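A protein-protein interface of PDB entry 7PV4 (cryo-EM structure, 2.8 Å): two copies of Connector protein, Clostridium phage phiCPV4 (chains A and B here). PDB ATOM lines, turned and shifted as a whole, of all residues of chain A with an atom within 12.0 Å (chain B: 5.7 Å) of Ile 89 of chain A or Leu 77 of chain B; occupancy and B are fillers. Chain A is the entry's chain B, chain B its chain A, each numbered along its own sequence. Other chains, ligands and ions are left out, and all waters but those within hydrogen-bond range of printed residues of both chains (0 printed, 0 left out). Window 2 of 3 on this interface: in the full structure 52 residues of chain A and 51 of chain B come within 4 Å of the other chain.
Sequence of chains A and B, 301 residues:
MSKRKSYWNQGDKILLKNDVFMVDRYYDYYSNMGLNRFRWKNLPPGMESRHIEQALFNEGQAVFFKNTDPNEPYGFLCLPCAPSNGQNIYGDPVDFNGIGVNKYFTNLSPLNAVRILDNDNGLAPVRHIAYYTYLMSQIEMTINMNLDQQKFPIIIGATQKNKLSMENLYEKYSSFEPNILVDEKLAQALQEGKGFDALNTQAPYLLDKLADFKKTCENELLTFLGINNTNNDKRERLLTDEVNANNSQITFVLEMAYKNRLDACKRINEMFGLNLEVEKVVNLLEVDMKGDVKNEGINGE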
ATOM      1  N   ASN A  85     -11.083  14.314 -31.448  1.00  0.00           N
ATOM      2  CA  ASN A  85     -12.414  14.085 -30.869  1.00  0.00           C
ATOM      3  C   ASN A  85     -12.530  14.308 -29.340  1.00  0.00           C
ATOM      4  O   ASN A  85     -13.641  14.306 -28.816  1.00  0.00           O
ATOM      5  CB  ASN A  85     -12.908  12.674 -31.261  1.00  0.00           C
ATOM      6  CG  ASN A  85     -13.195  12.454 -32.740  1.00  0.00           C
ATOM      7  OD1 ASN A  85     -12.906  11.412 -33.309  1.00  0.00           O
ATOM      8  ND2 ASN A  85     -13.793  13.403 -33.413  1.00  0.00           N
ATOM      9  N   GLY A  86     -11.435  14.507 -28.603  1.00  0.00           N
ATOM     10  CA  GLY A  86     -11.470  14.808 -27.164  1.00  0.00           C
ATOM     11  C   GLY A  86     -11.693  16.291 -26.873  1.00  0.00           C
ATOM     12  O   GLY A  86     -11.262  17.142 -27.643  1.00  0.00           O
ATOM     13  N   GLN A  87     -12.349  16.620 -25.761  1.00  0.00           N
ATOM     14  CA  GLN A  87     -12.762  17.988 -25.415  1.00  0.00           C
ATOM     15  C   GLN A  87     -12.873  18.252 -23.899  1.00  0.00           C
ATOM     16  O   GLN A  87     -13.089  17.329 -23.113  1.00  0.00           O
ATOM     17  CB  GLN A  87     -14.058  18.325 -26.161  1.00  0.00           C
ATOM     18  CG  GLN A  87     -15.194  17.312 -25.980  1.00  0.00           C
ATOM     19  CD  GLN A  87     -16.443  17.660 -26.788  1.00  0.00           C
ATOM     20  OE1 GLN A  87     -16.488  18.585 -27.572  1.00  0.00           O
ATOM     21  NE2 GLN A  87     -17.516  16.926 -26.648  1.00  0.00           N
ATOM     22  N   ASN A  88     -12.738  19.510 -23.472  1.00  0.00           N
ATOM     23  CA  ASN A  88     -12.952  19.926 -22.075  1.00  0.00           C
ATOM     24  C   ASN A  88     -14.451  19.976 -21.665  1.00  0.00           C
ATOM     25  O   ASN A  88     -15.331  19.655 -22.459  1.00  0.00           O
ATOM     26  CB  ASN A  88     -12.201  21.252 -21.822  1.00  0.00           C
ATOM     27  CG  ASN A  88     -12.792  22.477 -22.490  1.00  0.00           C
ATOM     28  OD1 ASN A  88     -13.877  22.463 -23.030  1.00  0.00           O
ATOM     29  ND2 ASN A  88     -12.103  23.583 -22.465  1.00  0.00           N
ATOM     30  N   ILE A  89     -14.759  20.413 -20.435  1.00  0.00           N
ATOM     31  CA  ILE A  89     -16.143  20.574 -19.926  1.00  0.00           C
ATOM     32  C   ILE A  89     -17.047  21.418 -20.832  1.00  0.00           C
ATOM     33  O   ILE A  89     -18.214  21.091 -21.006  1.00  0.00           O
ATOM     34  CB  ILE A  89     -16.179  21.181 -18.497  1.00  0.00           C
ATOM     35  CG1 ILE A  89     -15.214  22.371 -18.297  1.00  0.00           C
ATOM     36  CG2 ILE A  89     -15.954  20.096 -17.436  1.00  0.00           C
ATOM     37  CD1 ILE A  89     -15.577  23.286 -17.120  1.00  0.00           C
ATOM     38  N   TYR A  90     -16.523  22.491 -21.418  1.00  0.00           N
ATOM     39  CA  TYR A  90     -17.246  23.385 -22.311  1.00  0.00           C
ATOM     40  C   TYR A  90     -17.426  22.840 -23.735  1.00  0.00           C
ATOM     41  O   TYR A  90     -18.262  23.332 -24.478  1.00  0.00           O
ATOM     42  CB  TYR A  90     -16.507  24.724 -22.338  1.00  0.00           C
ATOM     43  CG  TYR A  90     -16.383  25.415 -20.996  1.00  0.00           C
ATOM     44  CD1 TYR A  90     -17.544  25.796 -20.306  1.00  0.00           C
ATOM     45  CD2 TYR A  90     -15.121  25.734 -20.463  1.00  0.00           C
ATOM     46  CE1 TYR A  90     -17.452  26.468 -19.075  1.00  0.00           C
ATOM     47  CE2 TYR A  90     -15.024  26.417 -19.237  1.00  0.00           C
ATOM     48  CZ  TYR A  90     -16.192  26.772 -18.533  1.00  0.00           C
ATOM     49  OH  TYR A  90     -16.110  27.409 -17.342  1.00  0.00           O
ATOM     50  N   GLY A  91     -16.646  21.838 -24.132  1.00  0.00           N
ATOM     51  CA  GLY A  91     -16.632  21.285 -25.481  1.00  0.00           C
ATOM     52  C   GLY A  91     -15.572  21.881 -26.405  1.00  0.00           C
ATOM     53  O   GLY A  91     -15.676  21.750 -27.618  1.00  0.00           O
ATOM     54  N   ASP A  92     -14.555  22.555 -25.875  1.00  0.00           N
ATOM     55  CA  ASP A  92     -13.393  22.950 -26.675  1.00  0.00           C
ATOM     56  C   ASP A  92     -12.520  21.723 -26.990  1.00  0.00           C
ATOM     57  O   ASP A  92     -12.216  20.963 -26.068  1.00  0.00           O
ATOM     58  CB  ASP A  92     -12.526  23.975 -25.947  1.00  0.00           C
ATOM     59  CG  ASP A  92     -13.240  25.246 -25.489  1.00  0.00           C
ATOM     60  OD1 ASP A  92     -12.818  25.811 -24.456  1.00  0.00           O
ATOM     61  OD2 ASP A  92     -14.159  25.724 -26.183  1.00  0.00           O
ATOM     62  N   PRO A  93     -12.061  21.514 -28.239  1.00  0.00           N
ATOM     63  CA  PRO A  93     -11.200  20.386 -28.570  1.00  0.00           C
ATOM     64  C   PRO A  93      -9.816  20.505 -27.914  1.00  0.00           C
ATOM     65  O   PRO A  93      -9.230  21.580 -27.871  1.00  0.00           O
ATOM     66  CB  PRO A  93     -11.139  20.346 -30.096  1.00  0.00           C
ATOM     67  CG  PRO A  93     -11.383  21.797 -30.504  1.00  0.00           C
ATOM     68  CD  PRO A  93     -12.298  22.335 -29.411  1.00  0.00           C
ATOM     69  N   VAL A  94      -9.277  19.401 -27.398  1.00  0.00           N
ATOM     70  CA  VAL A  94      -7.993  19.418 -26.662  1.00  0.00           C
ATOM     71  C   VAL A  94      -6.758  19.514 -27.559  1.00  0.00           C
ATOM     72  O   VAL A  94      -5.752  20.048 -27.121  1.00  0.00           O
ATOM     73  CB  VAL A  94      -7.853  18.224 -25.698  1.00  0.00           C
ATOM     74  CG1 VAL A  94      -8.975  18.202 -24.662  1.00  0.00           C
ATOM     75  CG2 VAL A  94      -7.807  16.860 -26.398  1.00  0.00           C
ATOM     76  N   ASP A  95      -6.819  19.052 -28.810  1.00  0.00           N
ATOM     77  CA  ASP A  95      -5.721  19.061 -29.790  1.00  0.00           C
ATOM     78  C   ASP A  95      -6.225  19.331 -31.220  1.00  0.00           C
ATOM     79  O   ASP A  95      -7.387  19.086 -31.542  1.00  0.00           O
ATOM     80  CB  ASP A  95      -4.926  17.745 -29.754  1.00  0.00           C
ATOM     81  CG  ASP A  95      -4.140  17.511 -28.458  1.00  0.00           C
ATOM     82  OD1 ASP A  95      -4.420  16.511 -27.765  1.00  0.00           O
ATOM     83  OD2 ASP A  95      -3.202  18.274 -28.154  1.00  0.00           O
ATOM     84  N   PRO A 110      -3.405  23.869 -27.956  1.00  0.00           N
ATOM     85  CA  PRO A 110      -3.616  25.261 -27.568  1.00  0.00           C
ATOM     86  C   PRO A 110      -2.427  25.892 -26.833  1.00  0.00           C
ATOM     87  O   PRO A 110      -2.359  27.108 -26.718  1.00  0.00           O
ATOM     88  CB  PRO A 110      -4.863  25.258 -26.683  1.00  0.00           C
ATOM     89  CG  PRO A 110      -5.564  23.946 -26.979  1.00  0.00           C
ATOM     90  CD  PRO A 110      -4.425  23.027 -27.380  1.00  0.00           C
ATOM     91  N   MET B  47     -11.818  31.460 -18.275  1.00  0.00           N
ATOM     92  CA  MET B  47     -13.214  31.507 -18.716  1.00  0.00           C
ATOM     93  C   MET B  47     -13.461  32.654 -19.703  1.00  0.00           C
ATOM     94  O   MET B  47     -12.888  33.729 -19.578  1.00  0.00           O
ATOM     95  CB  MET B  47     -14.089  31.600 -17.467  1.00  0.00           C
ATOM     96  CG  MET B  47     -15.565  31.337 -17.731  1.00  0.00           C
ATOM     97  SD  MET B  47     -16.542  31.227 -16.215  1.00  0.00           S
ATOM     98  CE  MET B  47     -16.696  32.972 -15.872  1.00  0.00           C
ATOM     99  N   VAL B  63     -25.952  28.010 -14.512  1.00  0.00           N
ATOM    100  CA  VAL B  63     -25.550  28.108 -13.103  1.00  0.00           C
ATOM    101  C   VAL B  63     -24.071  28.464 -12.978  1.00  0.00           C
ATOM    102  O   VAL B  63     -23.221  27.801 -13.563  1.00  0.00           O
ATOM    103  CB  VAL B  63     -25.974  26.852 -12.315  1.00  0.00           C
ATOM    104  CG1 VAL B  63     -25.359  25.537 -12.807  1.00  0.00           C
ATOM    105  CG2 VAL B  63     -25.698  27.019 -10.824  1.00  0.00           C
ATOM    106  N   PHE B  64     -23.781  29.513 -12.206  1.00  0.00           N
ATOM    107  CA  PHE B  64     -22.444  30.033 -11.909  1.00  0.00           C
ATOM    108  C   PHE B  64     -22.048  29.654 -10.476  1.00  0.00           C
ATOM    109  O   PHE B  64     -22.759  29.981  -9.525  1.00  0.00           O
ATOM    110  CB  PHE B  64     -22.487  31.556 -12.095  1.00  0.00           C
ATOM    111  CG  PHE B  64     -21.166  32.298 -12.123  1.00  0.00           C
ATOM    112  CD1 PHE B  64     -20.747  32.904 -13.320  1.00  0.00           C
ATOM    113  CD2 PHE B  64     -20.376  32.432 -10.966  1.00  0.00           C
ATOM    114  CE1 PHE B  64     -19.533  33.601 -13.373  1.00  0.00           C
ATOM    115  CE2 PHE B  64     -19.159  33.128 -11.023  1.00  0.00           C
ATOM    116  CZ  PHE B  64     -18.737  33.712 -12.227  1.00  0.00           C
ATOM    117  N   PHE B  65     -20.924  28.958 -10.306  1.00  0.00           N
ATOM    118  CA  PHE B  65     -20.470  28.439  -9.011  1.00  0.00           C
ATOM    119  C   PHE B  65     -18.945  28.260  -8.938  1.00  0.00           C
ATOM    120  O   PHE B  65     -18.255  28.103  -9.942  1.00  0.00           O
ATOM    121  CB  PHE B  65     -21.195  27.115  -8.708  1.00  0.00           C
ATOM    122  CG  PHE B  65     -20.934  25.991  -9.694  1.00  0.00           C
ATOM    123  CD1 PHE B  65     -21.579  25.996 -10.942  1.00  0.00           C
ATOM    124  CD2 PHE B  65     -20.045  24.946  -9.386  1.00  0.00           C
ATOM    125  CE1 PHE B  65     -21.296  25.009 -11.894  1.00  0.00           C
ATOM    126  CE2 PHE B  65     -19.792  23.937 -10.330  1.00  0.00           C
ATOM    127  CZ  PHE B  65     -20.392  23.982 -11.596  1.00  0.00           C
ATOM    128  N   LYS B  66     -18.409  28.256  -7.717  1.00  0.00           N
ATOM    129  CA  LYS B  66     -17.008  27.957  -7.400  1.00  0.00           C
ATOM    130  C   LYS B  66     -16.735  26.450  -7.516  1.00  0.00           C
ATOM    131  O   LYS B  66     -17.461  25.641  -6.937  1.00  0.00           O
ATOM    132  CB  LYS B  66     -16.769  28.489  -5.977  1.00  0.00           C
ATOM    133  CG  LYS B  66     -15.325  28.407  -5.475  1.00  0.00           C
ATOM    134  CD  LYS B  66     -14.449  29.556  -5.992  1.00  0.00           C
ATOM    135  CE  LYS B  66     -13.002  29.467  -5.495  1.00  0.00           C
ATOM    136  NZ  LYS B  66     -12.318  28.237  -5.970  1.00  0.00           N
ATOM    137  N   ASN B  67     -15.682  26.055  -8.234  1.00  0.00           N
ATOM    138  CA  ASN B  67     -15.299  24.649  -8.385  1.00  0.00           C
ATOM    139  C   ASN B  67     -14.702  24.079  -7.086  1.00  0.00           C
ATOM    140  O   ASN B  67     -13.952  24.756  -6.385  1.00  0.00           O
ATOM    141  CB  ASN B  67     -14.302  24.515  -9.548  1.00  0.00           C
ATOM    142  CG  ASN B  67     -13.851  23.078  -9.765  1.00  0.00           C
ATOM    143  OD1 ASN B  67     -14.588  22.130  -9.530  1.00  0.00           O
ATOM    144  ND2 ASN B  67     -12.622  22.868 -10.158  1.00  0.00           N
ATOM    145  N   GLU B  72     -10.293  19.252 -12.091  1.00  0.00           N
ATOM    146  CA  GLU B  72     -10.710  20.181 -13.141  1.00  0.00           C
ATOM    147  C   GLU B  72      -9.980  21.532 -12.978  1.00  0.00           C
ATOM    148  O   GLU B  72      -9.978  22.094 -11.883  1.00  0.00           O
ATOM    149  CB  GLU B  72     -12.237  20.329 -13.144  1.00  0.00           C
ATOM    150  CG  GLU B  72     -13.057  19.032 -13.014  1.00  0.00           C
ATOM    151  CD  GLU B  72     -12.727  17.937 -14.043  1.00  0.00           C
ATOM    152  OE1 GLU B  72     -12.228  18.242 -15.133  1.00  0.00           O
ATOM    153  OE2 GLU B  72     -13.034  16.764 -13.781  1.00  0.00           O
ATOM    154  N   TYR B  74     -10.070  24.716 -13.058  1.00  0.00           N
ATOM    155  CA  TYR B  74     -10.913  25.912 -13.009  1.00  0.00           C
ATOM    156  C   TYR B  74     -11.177  26.346 -11.579  1.00  0.00           C
ATOM    157  O   TYR B  74     -11.354  25.512 -10.696  1.00  0.00           O
ATOM    158  CB  TYR B  74     -12.236  25.667 -13.749  1.00  0.00           C
ATOM    159  CG  TYR B  74     -12.029  25.316 -15.204  1.00  0.00           C
ATOM    160  CD1 TYR B  74     -11.656  26.321 -16.119  1.00  0.00           C
ATOM    161  CD2 TYR B  74     -12.126  23.977 -15.623  1.00  0.00           C
ATOM    162  CE1 TYR B  74     -11.371  25.989 -17.454  1.00  0.00           C
ATOM    163  CE2 TYR B  74     -11.852  23.643 -16.962  1.00  0.00           C
ATOM    164  CZ  TYR B  74     -11.458  24.648 -17.870  1.00  0.00           C
ATOM    165  OH  TYR B  74     -11.122  24.313 -19.140  1.00  0.00           O
ATOM    166  N   GLY B  75     -11.238  27.659 -11.375  1.00  0.00           N
ATOM    167  CA  GLY B  75     -11.645  28.276 -10.112  1.00  0.00           C
ATOM    168  C   GLY B  75     -13.160  28.429  -9.993  1.00  0.00           C
ATOM    169  O   GLY B  75     -13.748  28.076  -8.976  1.00  0.00           O
ATOM    170  N   PHE B  76     -13.791  28.873 -11.071  1.00  0.00           N
ATOM    171  CA  PHE B  76     -15.225  29.062 -11.216  1.00  0.00           C
ATOM    172  C   PHE B  76     -15.709  28.455 -12.527  1.00  0.00           C
ATOM    173  O   PHE B  76     -15.003  28.510 -13.528  1.00  0.00           O
ATOM    174  CB  PHE B  76     -15.554  30.558 -11.213  1.00  0.00           C
ATOM    175  CG  PHE B  76     -15.319  31.274  -9.902  1.00  0.00           C
ATOM    176  CD1 PHE B  76     -16.360  31.366  -8.967  1.00  0.00           C
ATOM    177  CD2 PHE B  76     -14.084  31.874  -9.615  1.00  0.00           C
ATOM    178  CE1 PHE B  76     -16.172  32.050  -7.758  1.00  0.00           C
ATOM    179  CE2 PHE B  76     -13.895  32.580  -8.413  1.00  0.00           C
ATOM    180  CZ  PHE B  76     -14.944  32.665  -7.484  1.00  0.00           C
ATOM    181  N   LEU B  77     -16.931  27.935 -12.539  1.00  0.00           N
ATOM    182  CA  LEU B  77     -17.599  27.376 -13.717  1.00  0.00           C
ATOM    183  C   LEU B  77     -18.941  28.062 -13.956  1.00  0.00           C
ATOM    184  O   LEU B  77     -19.620  28.441 -13.012  1.00  0.00           O
ATOM    185  CB  LEU B  77     -17.789  25.859 -13.534  1.00  0.00           C
ATOM    186  CG  LEU B  77     -16.499  25.038 -13.443  1.00  0.00           C
ATOM    187  CD1 LEU B  77     -16.837  23.569 -13.225  1.00  0.00           C
ATOM    188  CD2 LEU B  77     -15.687  25.178 -14.719  1.00  0.00           C
ATOM    189  N   CYS B  78     -19.346  28.187 -15.218  1.00  0.00           N
ATOM    190  CA  CYS B  78     -20.688  28.608 -15.613  1.00  0.00           C
ATOM    191  C   CYS B  78     -21.235  27.633 -16.652  1.00  0.00           C
ATOM    192  O   CYS B  78     -20.720  27.577 -17.758  1.00  0.00           O
ATOM    193  CB  CYS B  78     -20.654  30.051 -16.115  1.00  0.00           C
ATOM    194  SG  CYS B  78     -22.342  30.622 -16.436  1.00  0.00           S
ATOM    195  N   LEU B  79     -22.234  26.832 -16.297  1.00  0.00           N
ATOM    196  CA  LEU B  79     -22.695  25.678 -17.083  1.00  0.00           C
ATOM    197  C   LEU B  79     -24.215  25.686 -17.258  1.00  0.00           C
ATOM    198  O   LEU B  79     -24.894  26.313 -16.453  1.00  0.00           O
ATOM    199  CB  LEU B  79     -22.222  24.384 -16.389  1.00  0.00           C
ATOM    200  CG  LEU B  79     -20.707  24.136 -16.431  1.00  0.00           C
ATOM    201  CD1 LEU B  79     -20.385  22.898 -15.607  1.00  0.00           C
ATOM    202  CD2 LEU B  79     -20.187  23.913 -17.854  1.00  0.00           C
ATOM    203  N   GLY B 100     -22.037  19.468 -17.418  1.00  0.00           N
ATOM    204  CA  GLY B 100     -20.835  19.681 -18.240  1.00  0.00           C
ATOM    205  C   GLY B 100     -20.639  18.593 -19.300  1.00  0.00           C
ATOM    206  O   GLY B 100     -21.288  17.556 -19.260  1.00  0.00           O
ATOM    207  N   VAL B 101     -19.738  18.786 -20.262  1.00  0.00           N
ATOM    208  CA  VAL B 101     -19.341  17.699 -21.180  1.00  0.00           C
ATOM    209  C   VAL B 101     -18.553  16.645 -20.394  1.00  0.00           C
ATOM    210  O   VAL B 101     -17.558  16.973 -19.759  1.00  0.00           O
ATOM    211  CB  VAL B 101     -18.553  18.232 -22.389  1.00  0.00           C
ATOM    212  CG1 VAL B 101     -18.000  17.101 -23.254  1.00  0.00           C
ATOM    213  CG2 VAL B 101     -19.440  19.109 -23.271  1.00  0.00           C
ATOM    214  N   LYS B 103     -19.343  15.412 -17.556  1.00  0.00           N
ATOM    215  CA  LYS B 103     -19.346  15.852 -16.151  1.00  0.00           C
ATOM    216  C   LYS B 103     -20.750  16.224 -15.674  1.00  0.00           C
ATOM    217  O   LYS B 103     -21.606  16.574 -16.472  1.00  0.00           O
ATOM    218  CB  LYS B 103     -18.365  17.028 -16.023  1.00  0.00           C
ATOM    219  CG  LYS B 103     -17.793  17.237 -14.621  1.00  0.00           C
ATOM    220  CD  LYS B 103     -16.733  16.199 -14.252  1.00  0.00           C
ATOM    221  CE  LYS B 103     -16.293  16.419 -12.806  1.00  0.00           C
ATOM    222  NZ  LYS B 103     -15.142  15.561 -12.463  1.00  0.00           N
ATOM    223  N   PHE B 105     -22.487  18.072 -11.928  1.00  0.00           N
ATOM    224  CA  PHE B 105     -22.301  18.596 -10.574  1.00  0.00           C
ATOM    225  C   PHE B 105     -23.617  18.489  -9.800  1.00  0.00           C
ATOM    226  O   PHE B 105     -24.626  19.088 -10.172  1.00  0.00           O
ATOM    227  CB  PHE B 105     -21.760  20.029 -10.638  1.00  0.00           C
ATOM    228  CG  PHE B 105     -20.385  20.126 -11.270  1.00  0.00           C
ATOM    229  CD1 PHE B 105     -20.233  20.328 -12.653  1.00  0.00           C
ATOM    230  CD2 PHE B 105     -19.238  19.956 -10.476  1.00  0.00           C
ATOM    231  CE1 PHE B 105     -18.958  20.326 -13.240  1.00  0.00           C
ATOM    232  CE2 PHE B 105     -17.960  19.962 -11.058  1.00  0.00           C
ATOM    233  CZ  PHE B 105     -17.820  20.142 -12.440  1.00  0.00           C
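O of Leu 79 of chain B lies within hydrogen-bond range of N of Val 63 of chain B, at 2.8 Å.
The backbone NH of Leu 77 of chain B lies within hydrogen-bond range of the backbone carbonyl oxygen of Phe 65 of chain B, at 2.9 Å.
The side-chain amide nitrogen of Asn 67 of chain B sits at hydrogen-bond distance from the backbone carbonyl oxygen of Tyr 74 of chain B (3.0 Å).
The backbone NH (N) of Tyr 90 of chain A is in hydrogen-bond range of the side-chain amide oxygen (OD1) of Asn 88 of chain A.
The side-chain amide oxygen of Asn 88 of chain A sits at hydrogen-bond distance from the backbone NH of Gly 91 of chain A.
OD1 of Asn 88 of chain A lies within hydrogen-bond range of N of Asp 92 of chain A (2.9 Å).
Printed residues of chain A within 4 Å of Leu 77 of chain B: Ile 89 (3.1 Å) and Tyr 90 (3.5 Å).
No residue of chain A comes within 4 Å of Val 63 of chain B.
No residue of chain A comes within 4 Å of Phe 64 of chain B.
No residue of chain A comes within 4 Å of Phe 65 of chain B.
No residue of chain A comes within 4 Å of Asn 67 of chain B.
Tyr 74 of chain B touches just these residues of chain A: Asn 88 and Ile 89.
No residue of chain A comes within 4 Å of Gly 75 of chain B.
Leu 79 of chain B touches just one residue of chain A: Tyr 90 (3.9 Å).
Gly 100 of chain B touches one residue of chain A.
No residue of chain A comes within 4 Å of Lys 103 of chain B.
Of the printed residues of chain B, Gln 87 of chain A touches Val 101.
Of the printed residues of chain B, Asn 88 of chain A touches Tyr 74 and Val 101.
Of the printed residues of chain A, Met 47 of chain B touches Tyr 90.
Printed residues of chain B within 4 Å of Tyr 90 of chain A: Met 47, Leu 77, Cys 78 and Leu 79.
Phe 105 of chain B touches none of the printed residues of chain A.
Val 94 of chain A touches none of the printed residues of chain B.
The nearest residue of chain B that does not touch Ile 89 of chain A is Lys 103 of chain B (4.1 Å).
No position is printed for both chains.
Of the 12 pairs that touch across the chains among the printed residues, none has its exchanged pair printed and touching as well.
Among the printed residues, pairs that only touch across the chains: Gln 87 of chain A with Val 101 of chain B, Asn 88 of chain A with Tyr 74 of chain B, Asn 88 of chain A with Val 101 of chain B, Ile 89 of chain A with Tyr 74 of chain B, Ile 89 of chain A with Leu 77 of chain B, Ile 89 of chain A with Gly 100 of chain B, Tyr 90 of chain A with Met 47 of chain B, Tyr 90 of chain A with Leu 77 of chain B, Tyr 90 of chain A with Cys 78 of chain B, Tyr 90 of chain A with Leu 79 of chain B and Gly 91 of chain A with Val 101 of chain B.
N of Val 101 of chain B sits at hydrogen-bond distance from O of Ile 89 of chain A (2.9 Å).
Of the 17 printed residues of chain B, 7 touch a printed residue of chain A.
Hydrophobic or aromatic side chains of chain B that line the printed part of chain A: Met 47, Tyr 74, Leu 77, Leu 79 and Val 101.
Along chain B the printed residues that touch a printed residue of chain A span positions 47 to 101.
Printed residues of chain A that touch a printed residue of chain B: Gln 87, Asn 88, Ile 89, Tyr 90 and Gly 91.
Hydrophobic or aromatic side chains of chain A within 4 Å of the printed part of chain B: Ile 89 and Tyr 90.
Along chain A the printed residues that touch a printed residue of chain B span positions 87 to 91.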
